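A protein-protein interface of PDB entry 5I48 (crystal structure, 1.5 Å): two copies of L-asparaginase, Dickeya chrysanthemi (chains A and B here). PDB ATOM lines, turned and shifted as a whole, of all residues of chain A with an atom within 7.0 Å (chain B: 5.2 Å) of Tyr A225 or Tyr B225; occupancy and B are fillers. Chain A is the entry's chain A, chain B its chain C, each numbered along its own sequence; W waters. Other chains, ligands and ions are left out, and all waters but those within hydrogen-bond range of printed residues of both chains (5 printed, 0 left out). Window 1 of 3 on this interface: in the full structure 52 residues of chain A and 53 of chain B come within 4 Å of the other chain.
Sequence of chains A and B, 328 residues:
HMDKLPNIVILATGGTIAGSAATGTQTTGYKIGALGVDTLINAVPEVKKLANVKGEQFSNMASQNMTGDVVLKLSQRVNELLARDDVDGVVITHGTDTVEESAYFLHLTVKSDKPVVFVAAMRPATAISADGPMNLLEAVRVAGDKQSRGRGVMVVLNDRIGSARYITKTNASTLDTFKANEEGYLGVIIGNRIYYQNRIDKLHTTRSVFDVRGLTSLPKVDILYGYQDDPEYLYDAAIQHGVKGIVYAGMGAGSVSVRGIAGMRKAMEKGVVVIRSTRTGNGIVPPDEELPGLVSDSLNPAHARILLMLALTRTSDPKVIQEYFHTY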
ATOM      1  N   ILE A 223     -30.464   5.308  20.215  1.00  0.00           N
ATOM      2  CA  ILE A 223     -30.015   4.388  19.161  1.00  0.00           C
ATOM      3  C   ILE A 223     -30.988   3.200  19.168  1.00  0.00           C
ATOM      4  O   ILE A 223     -31.221   2.591  20.194  1.00  0.00           O
ATOM      5  CB  ILE A 223     -28.586   3.842  19.413  1.00  0.00           C
ATOM      6  CG1 ILE A 223     -27.606   5.010  19.569  1.00  0.00           C
ATOM      7  CG2 ILE A 223     -28.197   2.894  18.284  1.00  0.00           C
ATOM      8  CD1 ILE A 223     -26.182   4.652  19.859  1.00  0.00           C
ATOM      9  N   LEU A 224     -31.513   2.892  17.962  1.00  0.00           N
ATOM     10  CA  LEU A 224     -32.427   1.798  17.781  1.00  0.00           C
ATOM     11  C   LEU A 224     -31.808   0.778  16.788  1.00  0.00           C
ATOM     12  O   LEU A 224     -31.203   1.138  15.804  1.00  0.00           O
ATOM     13  CB  LEU A 224     -33.765   2.253  17.179  1.00  0.00           C
ATOM     14  CG  LEU A 224     -34.544   3.181  18.092  1.00  0.00           C
ATOM     15  CD1 LEU A 224     -35.888   3.627  17.442  1.00  0.00           C
ATOM     16  CD2 LEU A 224     -34.819   2.488  19.434  1.00  0.00           C
ATOM     17  N   TYR A 225     -31.872  -0.481  17.171  1.00  0.00           N
ATOM     18  CA  TYR A 225     -31.324  -1.589  16.400  1.00  0.00           C
ATOM     19  C   TYR A 225     -32.245  -2.020  15.249  1.00  0.00           C
ATOM     20  O   TYR A 225     -33.433  -1.935  15.336  1.00  0.00           O
ATOM     21  CB  TYR A 225     -31.092  -2.780  17.286  1.00  0.00           C
ATOM     22  CG  TYR A 225     -29.913  -3.645  16.943  1.00  0.00           C
ATOM     23  CD1 TYR A 225     -28.631  -3.176  17.165  1.00  0.00           C
ATOM     24  CD2 TYR A 225     -30.046  -4.950  16.535  1.00  0.00           C
ATOM     25  CE1 TYR A 225     -27.524  -3.915  16.914  1.00  0.00           C
ATOM     26  CE2 TYR A 225     -28.903  -5.710  16.299  1.00  0.00           C
ATOM     27  CZ  TYR A 225     -27.642  -5.153  16.495  1.00  0.00           C
ATOM     28  OH  TYR A 225     -26.564  -5.989  16.259  1.00  0.00           O
ATOM     29  N   GLY A 226     -31.637  -2.468  14.178  1.00  0.00           N
ATOM     30  CA  GLY A 226     -32.354  -3.011  13.059  1.00  0.00           C
ATOM     31  C   GLY A 226     -32.109  -4.531  13.017  1.00  0.00           C
ATOM     32  O   GLY A 226     -30.993  -5.029  13.134  1.00  0.00           O
ATOM     33  N   TYR A 227     -33.212  -5.258  12.770  1.00  0.00           N
ATOM     34  CA  TYR A 227     -33.193  -6.719  12.760  1.00  0.00           C
ATOM     35  C   TYR A 227     -34.498  -7.205  12.191  1.00  0.00           C
ATOM     36  O   TYR A 227     -35.469  -6.433  12.071  1.00  0.00           O
ATOM     37  CB  TYR A 227     -32.960  -7.299  14.128  1.00  0.00           C
ATOM     38  CG  TYR A 227     -33.897  -6.764  15.227  1.00  0.00           C
ATOM     39  CD1 TYR A 227     -33.687  -5.503  15.788  1.00  0.00           C
ATOM     40  CD2 TYR A 227     -34.956  -7.495  15.682  1.00  0.00           C
ATOM     41  CE1 TYR A 227     -34.501  -4.998  16.798  1.00  0.00           C
ATOM     42  CE2 TYR A 227     -35.763  -7.020  16.697  1.00  0.00           C
ATOM     43  CZ  TYR A 227     -35.547  -5.774  17.249  1.00  0.00           C
ATOM     44  OH  TYR A 227     -36.322  -5.270  18.287  1.00  0.00           O
ATOM     45  N   ASP A 230     -38.126  -6.084  13.498  1.00  0.00           N
ATOM     46  CA  ASP A 230     -37.936  -4.918  14.323  1.00  0.00           C
ATOM     47  C   ASP A 230     -39.253  -4.113  14.480  1.00  0.00           C
ATOM     48  O   ASP A 230     -39.983  -3.894  13.492  1.00  0.00           O
ATOM     49  CB  ASP A 230     -36.815  -4.003  13.811  1.00  0.00           C
ATOM     50  CG  ASP A 230     -37.034  -3.434  12.435  1.00  0.00           C
ATOM     51  OD1 ASP A 230     -37.742  -4.013  11.538  1.00  0.00           O
ATOM     52  OD2 ASP A 230     -36.440  -2.371  12.210  1.00  0.00           O
ATOM     53  N   PRO A 231     -39.534  -3.614  15.693  1.00  0.00           N
ATOM     54  CA  PRO A 231     -40.848  -3.015  15.880  1.00  0.00           C
ATOM     55  C   PRO A 231     -40.923  -1.545  15.706  1.00  0.00           C
ATOM     56  O   PRO A 231     -40.064  -0.794  16.107  1.00  0.00           O
ATOM     57  CB  PRO A 231     -41.136  -3.331  17.315  1.00  0.00           C
ATOM     58  CG  PRO A 231     -39.742  -3.311  17.985  1.00  0.00           C
ATOM     59  CD  PRO A 231     -38.856  -3.919  16.964  1.00  0.00           C
ATOM     60  N   LEU A 234     -40.861   0.973  19.085  1.00  0.00           N
ATOM     61  CA  LEU A 234     -39.686   1.616  19.676  1.00  0.00           C
ATOM     62  C   LEU A 234     -39.429   2.995  19.129  1.00  0.00           C
ATOM     63  O   LEU A 234     -38.936   3.858  19.884  1.00  0.00           O
ATOM     64  CB  LEU A 234     -38.427   0.741  19.574  1.00  0.00           C
ATOM     65  CG  LEU A 234     -38.506  -0.574  20.378  1.00  0.00           C
ATOM     66  CD1 LEU A 234     -37.314  -1.423  20.025  1.00  0.00           C
ATOM     67  CD2 LEU A 234     -38.544  -0.363  21.869  1.00  0.00           C
ATOM     68  N   TYR A 235     -39.755   3.269  17.872  1.00  0.00           N
ATOM     69  CA  TYR A 235     -39.705   4.598  17.313  1.00  0.00           C
ATOM     70  C   TYR A 235     -40.735   5.457  18.012  1.00  0.00           C
ATOM     71  O   TYR A 235     -40.453   6.617  18.427  1.00  0.00           O
ATOM     72  CB  TYR A 235     -39.920   4.609  15.828  1.00  0.00           C
ATOM     73  CG  TYR A 235     -38.839   3.950  15.051  1.00  0.00           C
ATOM     74  CD1 TYR A 235     -38.834   2.577  14.865  1.00  0.00           C
ATOM     75  CD2 TYR A 235     -37.828   4.693  14.527  1.00  0.00           C
ATOM     76  CE1 TYR A 235     -37.770   1.953  14.242  1.00  0.00           C
ATOM     77  CE2 TYR A 235     -36.775   4.083  13.855  1.00  0.00           C
ATOM     78  CZ  TYR A 235     -36.791   2.727  13.681  1.00  0.00           C
ATOM     79  OH  TYR A 235     -35.731   2.122  13.030  1.00  0.00           O
ATOM     80  N   VAL A 247     -30.380   7.515  16.061  1.00  0.00           N
ATOM     81  CA  VAL A 247     -29.389   6.805  15.254  1.00  0.00           C
ATOM     82  C   VAL A 247     -29.878   5.375  15.100  1.00  0.00           C
ATOM     83  O   VAL A 247     -30.237   4.719  16.059  1.00  0.00           O
ATOM     84  CB  VAL A 247     -28.039   6.835  15.911  1.00  0.00           C
ATOM     85  CG1 VAL A 247     -27.057   5.903  15.193  1.00  0.00           C
ATOM     86  CG2 VAL A 247     -27.518   8.247  15.874  1.00  0.00           C
ATOM     87  N   TYR A 248     -29.971   4.917  13.860  1.00  0.00           N
ATOM     88  CA  TYR A 248     -30.425   3.577  13.562  1.00  0.00           C
ATOM     89  C   TYR A 248     -29.225   2.669  13.262  1.00  0.00           C
ATOM     90  O   TYR A 248     -28.487   2.914  12.289  1.00  0.00           O
ATOM     91  CB  TYR A 248     -31.334   3.730  12.351  1.00  0.00           C
ATOM     92  CG  TYR A 248     -31.761   2.440  11.700  1.00  0.00           C
ATOM     93  CD1 TYR A 248     -32.477   1.475  12.425  1.00  0.00           C
ATOM     94  CD2 TYR A 248     -31.462   2.198  10.364  1.00  0.00           C
ATOM     95  CE1 TYR A 248     -32.885   0.270  11.806  1.00  0.00           C
ATOM     96  CE2 TYR A 248     -31.910   1.015   9.740  1.00  0.00           C
ATOM     97  CZ  TYR A 248     -32.581   0.060  10.545  1.00  0.00           C
ATOM     98  OH  TYR A 248     -32.975  -1.111   9.958  1.00  0.00           O
ATOM     99  N   ALA A 249     -29.073   1.631  14.042  1.00  0.00           N
ATOM    100  CA  ALA A 249     -28.010   0.628  13.854  1.00  0.00           C
ATOM    101  C   ALA A 249     -28.572  -0.382  12.894  1.00  0.00           C
ATOM    102  O   ALA A 249     -29.039  -1.465  13.268  1.00  0.00           O
ATOM    103  CB  ALA A 249     -27.569  -0.011  15.169  1.00  0.00           C
ATOM    104  N   GLY A 250     -28.488  -0.022  11.650  1.00  0.00           N
ATOM    105  CA  GLY A 250     -29.246  -0.711  10.608  1.00  0.00           C
ATOM    106  C   GLY A 250     -28.751  -2.050  10.156  1.00  0.00           C
ATOM    107  O   GLY A 250     -27.596  -2.405  10.307  1.00  0.00           O
ATOM    108  N   MET A 251     -29.642  -2.775   9.520  1.00  0.00           N
ATOM    109  CA  MET A 251     -29.280  -3.979   8.848  1.00  0.00           C
ATOM    110  C   MET A 251     -28.428  -3.593   7.646  1.00  0.00           C
ATOM    111  O   MET A 251     -28.758  -2.702   6.930  1.00  0.00           O
ATOM    112  CB  MET A 251     -30.555  -4.753   8.398  1.00  0.00           C
ATOM    113  CG  MET A 251     -31.374  -5.215   9.610  1.00  0.00           C
ATOM    114  SD  MET A 251     -33.017  -5.815   9.192  1.00  0.00           S
ATOM    115  CE  MET A 251     -33.968  -4.287   9.219  1.00  0.00           C
ATOM    116  N   THR A 278     -25.119   1.494  10.765  1.00  0.00           N
ATOM    117  CA  THR A 278     -25.082   0.087  10.516  1.00  0.00           C
ATOM    118  C   THR A 278     -24.772  -0.711  11.761  1.00  0.00           C
ATOM    119  O   THR A 278     -23.928  -0.296  12.526  1.00  0.00           O
ATOM    120  CB  THR A 278     -24.087  -0.246   9.369  1.00  0.00           C
ATOM    121  OG1 THR A 278     -24.091  -1.671   9.124  1.00  0.00           O
ATOM    122  CG2 THR A 278     -22.675   0.195   9.657  1.00  0.00           C
ATOM    123  N   ARG A 279     -25.370  -1.877  11.913  1.00  0.00           N
ATOM    124  CA  ARG A 279     -25.050  -2.766  12.989  1.00  0.00           C
ATOM    125  C   ARG A 279     -23.807  -3.638  12.676  1.00  0.00           C
ATOM    126  O   ARG A 279     -23.385  -4.415  13.545  1.00  0.00           O
ATOM    127  CB  ARG A 279     -26.238  -3.715  13.345  1.00  0.00           C
ATOM    128  CG  ARG A 279     -26.445  -4.883  12.325  1.00  0.00           C
ATOM    129  CD  ARG A 279     -27.674  -5.671  12.594  1.00  0.00           C
ATOM    130  NE  ARG A 279     -27.639  -6.856  11.706  1.00  0.00           N
ATOM    131  CZ  ARG A 279     -28.610  -7.758  11.665  1.00  0.00           C
ATOM    132  NH1 ARG A 279     -29.710  -7.568  12.399  1.00  0.00           N
ATOM    133  NH2 ARG A 279     -28.524  -8.794  10.859  1.00  0.00           N
ATOM    134  N   THR A 280     -23.349  -3.606  11.421  1.00  0.00           N
ATOM    135  CA  THR A 280     -22.387  -4.575  10.967  1.00  0.00           C
ATOM    136  C   THR A 280     -21.029  -4.463  11.636  1.00  0.00           C
ATOM    137  O   THR A 280     -20.358  -5.517  11.814  1.00  0.00           O
ATOM    138  CB  THR A 280     -22.160  -4.505   9.449  1.00  0.00           C
ATOM    139  OG1 THR A 280     -21.698  -3.215   9.089  1.00  0.00           O
ATOM    140  CG2 THR A 280     -23.437  -4.832   8.679  1.00  0.00           C
ATOM    141  N   ASN A 300     -19.907   4.439  13.132  1.00  0.00           N
ATOM    142  CA  ASN A 300     -20.694   3.398  13.735  1.00  0.00           C
ATOM    143  C   ASN A 300     -21.755   3.994  14.629  1.00  0.00           C
ATOM    144  O   ASN A 300     -21.787   5.218  14.833  1.00  0.00           O
ATOM    145  CB  ASN A 300     -19.836   2.375  14.484  1.00  0.00           C
ATOM    146  CG  ASN A 300     -19.232   2.871  15.760  1.00  0.00           C
ATOM    147  OD1 ASN A 300     -19.538   3.907  16.331  1.00  0.00           O
ATOM    148  ND2 ASN A 300     -18.450   1.966  16.353  1.00  0.00           N
ATOM    149  N   PRO A 301     -22.690   3.174  15.135  1.00  0.00           N
ATOM    150  CA  PRO A 301     -23.772   3.831  15.861  1.00  0.00           C
ATOM    151  C   PRO A 301     -23.367   4.717  17.045  1.00  0.00           C
ATOM    152  O   PRO A 301     -23.944   5.797  17.250  1.00  0.00           O
ATOM    153  CB  PRO A 301     -24.697   2.683  16.252  1.00  0.00           C
ATOM    154  CG  PRO A 301     -24.458   1.686  15.130  1.00  0.00           C
ATOM    155  CD  PRO A 301     -22.974   1.792  14.871  1.00  0.00           C
ATOM    156  N   ALA A 302     -22.461   4.196  17.875  1.00  0.00           N
ATOM    157  CA  ALA A 302     -22.067   4.915  19.042  1.00  0.00           C
ATOM    158  C   ALA A 302     -21.421   6.270  18.681  1.00  0.00           C
ATOM    159  O   ALA A 302     -21.688   7.311  19.335  1.00  0.00           O
ATOM    160  CB  ALA A 302     -21.145   4.072  19.865  1.00  0.00           C
ATOM    161  N   ILE B 223     -34.446  -6.345  20.449  1.00  0.00           N
ATOM    162  CA  ILE B 223     -33.047  -6.099  20.745  1.00  0.00           C
ATOM    163  C   ILE B 223     -32.871  -4.663  21.096  1.00  0.00           C
ATOM    164  O   ILE B 223     -33.328  -3.774  20.334  1.00  0.00           O
ATOM    165  CB  ILE B 223     -32.140  -6.395  19.517  1.00  0.00           C
ATOM    166  CG1 ILE B 223     -32.328  -7.821  19.029  1.00  0.00           C
ATOM    167  CG2 ILE B 223     -30.670  -6.116  19.861  1.00  0.00           C
ATOM    168  CD1 ILE B 223     -31.576  -8.253  17.783  1.00  0.00           C
ATOM    169  N   LEU B 224     -32.253  -4.381  22.219  1.00  0.00           N
ATOM    170  CA  LEU B 224     -32.044  -3.006  22.668  1.00  0.00           C
ATOM    171  C   LEU B 224     -30.523  -2.760  22.756  1.00  0.00           C
ATOM    172  O   LEU B 224     -29.782  -3.575  23.225  1.00  0.00           O
ATOM    173  CB  LEU B 224     -32.669  -2.815  24.037  1.00  0.00           C
ATOM    174  CG  LEU B 224     -34.192  -2.920  24.108  1.00  0.00           C
ATOM    175  CD1 LEU B 224     -34.700  -2.711  25.561  1.00  0.00           C
ATOM    176  CD2 LEU B 224     -34.836  -1.954  23.150  1.00  0.00           C
ATOM    177  N   TYR B 225     -30.116  -1.609  22.296  1.00  0.00           N
ATOM    178  CA  TYR B 225     -28.724  -1.257  22.270  1.00  0.00           C
ATOM    179  C   TYR B 225     -28.254  -0.661  23.618  1.00  0.00           C
ATOM    180  O   TYR B 225     -28.985  -0.015  24.318  1.00  0.00           O
ATOM    181  CB  TYR B 225     -28.498  -0.162  21.200  1.00  0.00           C
ATOM    182  CG  TYR B 225     -27.157  -0.195  20.488  1.00  0.00           C
ATOM    183  CD1 TYR B 225     -26.862  -1.248  19.633  1.00  0.00           C
ATOM    184  CD2 TYR B 225     -26.257   0.827  20.598  1.00  0.00           C
ATOM    185  CE1 TYR B 225     -25.700  -1.308  18.988  1.00  0.00           C
ATOM    186  CE2 TYR B 225     -25.082   0.770  19.867  1.00  0.00           C
ATOM    187  CZ  TYR B 225     -24.835  -0.249  19.081  1.00  0.00           C
ATOM    188  OH  TYR B 225     -23.650  -0.268  18.350  1.00  0.00           O
ATOM    189  N   GLY B 226     -26.977  -0.859  23.898  1.00  0.00           N
ATOM    190  CA  GLY B 226     -26.341  -0.267  25.062  1.00  0.00           C
ATOM    191  C   GLY B 226     -25.341   0.780  24.617  1.00  0.00           C
ATOM    192  O   GLY B 226     -24.586   0.636  23.680  1.00  0.00           O
ATOM    193  N   TYR B 227     -25.373   1.912  25.313  1.00  0.00           N
ATOM    194  CA  TYR B 227     -24.608   3.104  24.971  1.00  0.00           C
ATOM    195  C   TYR B 227     -24.722   4.116  26.109  1.00  0.00           C
ATOM    196  O   TYR B 227     -25.600   4.005  26.993  1.00  0.00           O
ATOM    197  CB  TYR B 227     -25.097   3.754  23.699  1.00  0.00           C
ATOM    198  CG  TYR B 227     -26.595   4.072  23.619  1.00  0.00           C
ATOM    199  CD1 TYR B 227     -27.524   3.101  23.322  1.00  0.00           C
ATOM    200  CD2 TYR B 227     -27.057   5.380  23.767  1.00  0.00           C
ATOM    201  CE1 TYR B 227     -28.868   3.396  23.288  1.00  0.00           C
ATOM    202  CE2 TYR B 227     -28.384   5.662  23.666  1.00  0.00           C
ATOM    203  CZ  TYR B 227     -29.268   4.649  23.431  1.00  0.00           C
ATOM    204  OH  TYR B 227     -30.635   4.930  23.227  1.00  0.00           O
ATOM    205  N   ASP B 230     -28.185   5.501  27.770  1.00  0.00           N
ATOM    206  CA  ASP B 230     -29.210   4.625  27.274  1.00  0.00           C
ATOM    207  C   ASP B 230     -30.461   4.701  28.152  1.00  0.00           C
ATOM    208  O   ASP B 230     -30.355   4.730  29.359  1.00  0.00           O
ATOM    209  CB  ASP B 230     -28.783   3.172  27.134  1.00  0.00           C
ATOM    210  CG  ASP B 230     -28.274   2.548  28.401  1.00  0.00           C
ATOM    211  OD1 ASP B 230     -27.796   3.187  29.383  1.00  0.00           O
ATOM    212  OD2 ASP B 230     -28.396   1.297  28.420  1.00  0.00           O
ATOM    213  N   TYR B 248     -29.884  -7.850  24.716  1.00  0.00           N
ATOM    214  CA  TYR B 248     -29.199  -6.539  24.964  1.00  0.00           C
ATOM    215  C   TYR B 248     -27.887  -6.510  24.200  1.00  0.00           C
ATOM    216  O   TYR B 248     -27.019  -7.351  24.469  1.00  0.00           O
ATOM    217  CB  TYR B 248     -29.001  -6.388  26.440  1.00  0.00           C
ATOM    218  CG  TYR B 248     -28.144  -5.244  26.907  1.00  0.00           C
ATOM    219  CD1 TYR B 248     -28.487  -3.955  26.626  1.00  0.00           C
ATOM    220  CD2 TYR B 248     -26.960  -5.487  27.622  1.00  0.00           C
ATOM    221  CE1 TYR B 248     -27.707  -2.886  27.051  1.00  0.00           C
ATOM    222  CE2 TYR B 248     -26.203  -4.464  28.064  1.00  0.00           C
ATOM    223  CZ  TYR B 248     -26.542  -3.191  27.745  1.00  0.00           C
ATOM    224  OH  TYR B 248     -25.763  -2.128  28.147  1.00  0.00           O
ATOM    225  N   ALA B 249     -27.741  -5.553  23.271  1.00  0.00           N
ATOM    226  CA  ALA B 249     -26.487  -5.406  22.491  1.00  0.00           C
ATOM    227  C   ALA B 249     -25.622  -4.479  23.356  1.00  0.00           C
ATOM    228  O   ALA B 249     -25.569  -3.270  23.151  1.00  0.00           O
ATOM    229  CB  ALA B 249     -26.799  -4.802  21.143  1.00  0.00           C
ATOM    230  N   ARG B 279     -22.458  -5.234  21.675  1.00  0.00           N
ATOM    231  CA  ARG B 279     -22.518  -4.450  20.468  1.00  0.00           C
ATOM    232  C   ARG B 279     -21.166  -4.447  19.717  1.00  0.00           C
ATOM    233  O   ARG B 279     -21.054  -3.873  18.659  1.00  0.00           O
ATOM    234  CB  ARG B 279     -22.880  -2.948  20.801  1.00  0.00           C
ATOM    235  CG  ARG B 279     -21.701  -2.143  21.425  1.00  0.00           C
ATOM    236  CD  ARG B 279     -22.103  -0.766  21.900  1.00  0.00           C
ATOM    237  NE  ARG B 279     -20.919   0.004  22.243  1.00  0.00           N
ATOM    238  CZ  ARG B 279     -20.906   1.239  22.689  1.00  0.00           C
ATOM    239  NH1 ARG B 279     -21.986   1.837  22.910  1.00  0.00           N
ATOM    240  NH2 ARG B 279     -19.745   1.870  22.888  1.00  0.00           N
ATOM    241  N   PRO B 301     -25.863 -10.064  18.726  1.00  0.00           N
ATOM    242  CA  PRO B 301     -27.277  -9.813  19.042  1.00  0.00           C
ATOM    243  C   PRO B 301     -28.286 -10.430  18.102  1.00  0.00           C
ATOM    244  O   PRO B 301     -29.281 -11.025  18.599  1.00  0.00           O
ATOM    245  CB  PRO B 301     -27.357  -8.336  19.068  1.00  0.00           C
ATOM    246  CG  PRO B 301     -25.969  -7.871  19.489  1.00  0.00           C
ATOM    247  CD  PRO B 301     -25.066  -8.807  18.758  1.00  0.00           C
ATOM    248  N   ALA B 302     -28.007 -10.375  16.814  1.00  0.00           N
ATOM    249  CA  ALA B 302     -28.963 -10.917  15.829  1.00  0.00           C
ATOM    250  C   ALA B 302     -29.092 -12.456  16.008  1.00  0.00           C
ATOM    251  O   ALA B 302     -30.216 -12.975  15.977  1.00  0.00           O
ATOM    252  CB  ALA B 302     -28.498 -10.548  14.398  1.00  0.00           C
HETATM  253  O   HOH W   1     -32.111   0.324  21.428  1.00  0.00           O
HETATM  254  O   HOH W   2     -33.492  -1.182  19.535  1.00  0.00           O
HETATM  255  O   HOH W   3     -20.672  -4.659  15.472  1.00  0.00           O
HETATM  256  O   HOH W   4     -26.061  -8.526  15.577  1.00  0.00           O
HETATM  257  O   HOH W   5     -21.556   1.391  17.877  1.00  0.00           O
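The backbone carbonyl oxygen (O) of Gly A226 lies within hydrogen-bond range of the guanidinium group (NH1) of Arg A279 (2.9 Å).
SD of Met A251 sits close to N of Tyr A227 (3.6 Å).
The backbone carbonyl oxygen (O) of Gly A250 sits at hydrogen-bond distance from the backbone NH (N) of Arg A279.
N of Ala A302 is in hydrogen-bond range of OD1 of Asn A300, 3.3 Å away.
The backbone carbonyl oxygen of Gly B226 is in hydrogen-bond range of the guanidinium group of Arg B279, 3.0 Å away.
Ile A223 touches Tyr B225, and with the chains exchanged Tyr A225 touches Ile B223.
Ile A223 touches Tyr B227, and with the chains exchanged Tyr A227 touches Ile B223.
Tyr B225 touches its own counterpart, Tyr A225.
Tyr A225 touches Pro B301, and with the chains exchanged Pro A301 touches Tyr B225.
Of the 9 pairs that touch across the chains among the printed residues, 9 have their exchanged pair printed and touching as well.
Ile A223 touches Tyr B225 (CG2 to CD2, 3.7 Å).
Tyr A225 touches Ile B223 (CD2 to CG2, 3.6 Å).
CD1 of Tyr A225 touches CD1 of Tyr B225, at 3.6 Å.
Tyr A225 touches Pro B301 (OH to CB, 3.7 Å).
Ala B302 touches Arg A279.
CB of Pro A301 touches OH of Tyr B225, at 3.8 Å.
CB of Ala A302 touches NH1 of Arg B279 (3.9 Å).
Of the 20 printed residues of chain A, 6 touch a printed residue of chain B.
Hydrophobic or aromatic side chains of chain A within 4 Å of the printed part of chain B: Ile A223, Tyr A225, Tyr A227, Pro A301 and Ala A302.
Among the printed residues, no Asp or Glu carboxylate lies within 4 Å of a Lys or Arg side-chain nitrogen of the other chain.
Of chain B, only Ile B223, Tyr B225 and Pro B301 come within 4 Å of Tyr A225.
Printed residues of chain B within 4 Å of Arg A279: Ala B302 (3.8 Å).
Of chain A, only Ile A223, Tyr A225 and Pro A301 come within 4 Å of Tyr B225.
Of the printed residues of chain A, Tyr B227 touches Ile A223 (3.0 Å).
Of the printed residues of chain A, Pro B301 touches Tyr A225.
Of the printed residues of chain A, Ala B302 touches Arg A279 (3.8 Å).
The nearest residue of chain A that does not touch Tyr B225 is Ala A249 (4.4 Å).
The backbone NH (N) of Ile A223 lies within hydrogen-bond range of the side-chain hydroxyl (OH) of Tyr B227 (3.0 Å).
N of Ile B223 is in hydrogen-bond range of OH of Tyr A227.
Water W4 bridges OH of Tyr A225 (2.7 Å) and N of Ala B302 (3.0 Å).
Water W5 lies within hydrogen-bond range of the side-chain hydroxyl of Tyr B225 and the backbone NH of Ala A302.
Water W2 bridges the backbone carbonyl oxygen (O) of Ile B223 (2.7 Å) and the backbone NH (N) of Tyr A225 (3.0 Å).
Water W1 bridges the backbone carbonyl oxygen (O) of Ile A223 and the backbone NH (N) of Tyr B225.
Water W3 bridges the backbone carbonyl oxygen (O) of Arg B279 (3.3 Å) and the backbone carbonyl oxygen (O) of Arg A279 (3.3 Å).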
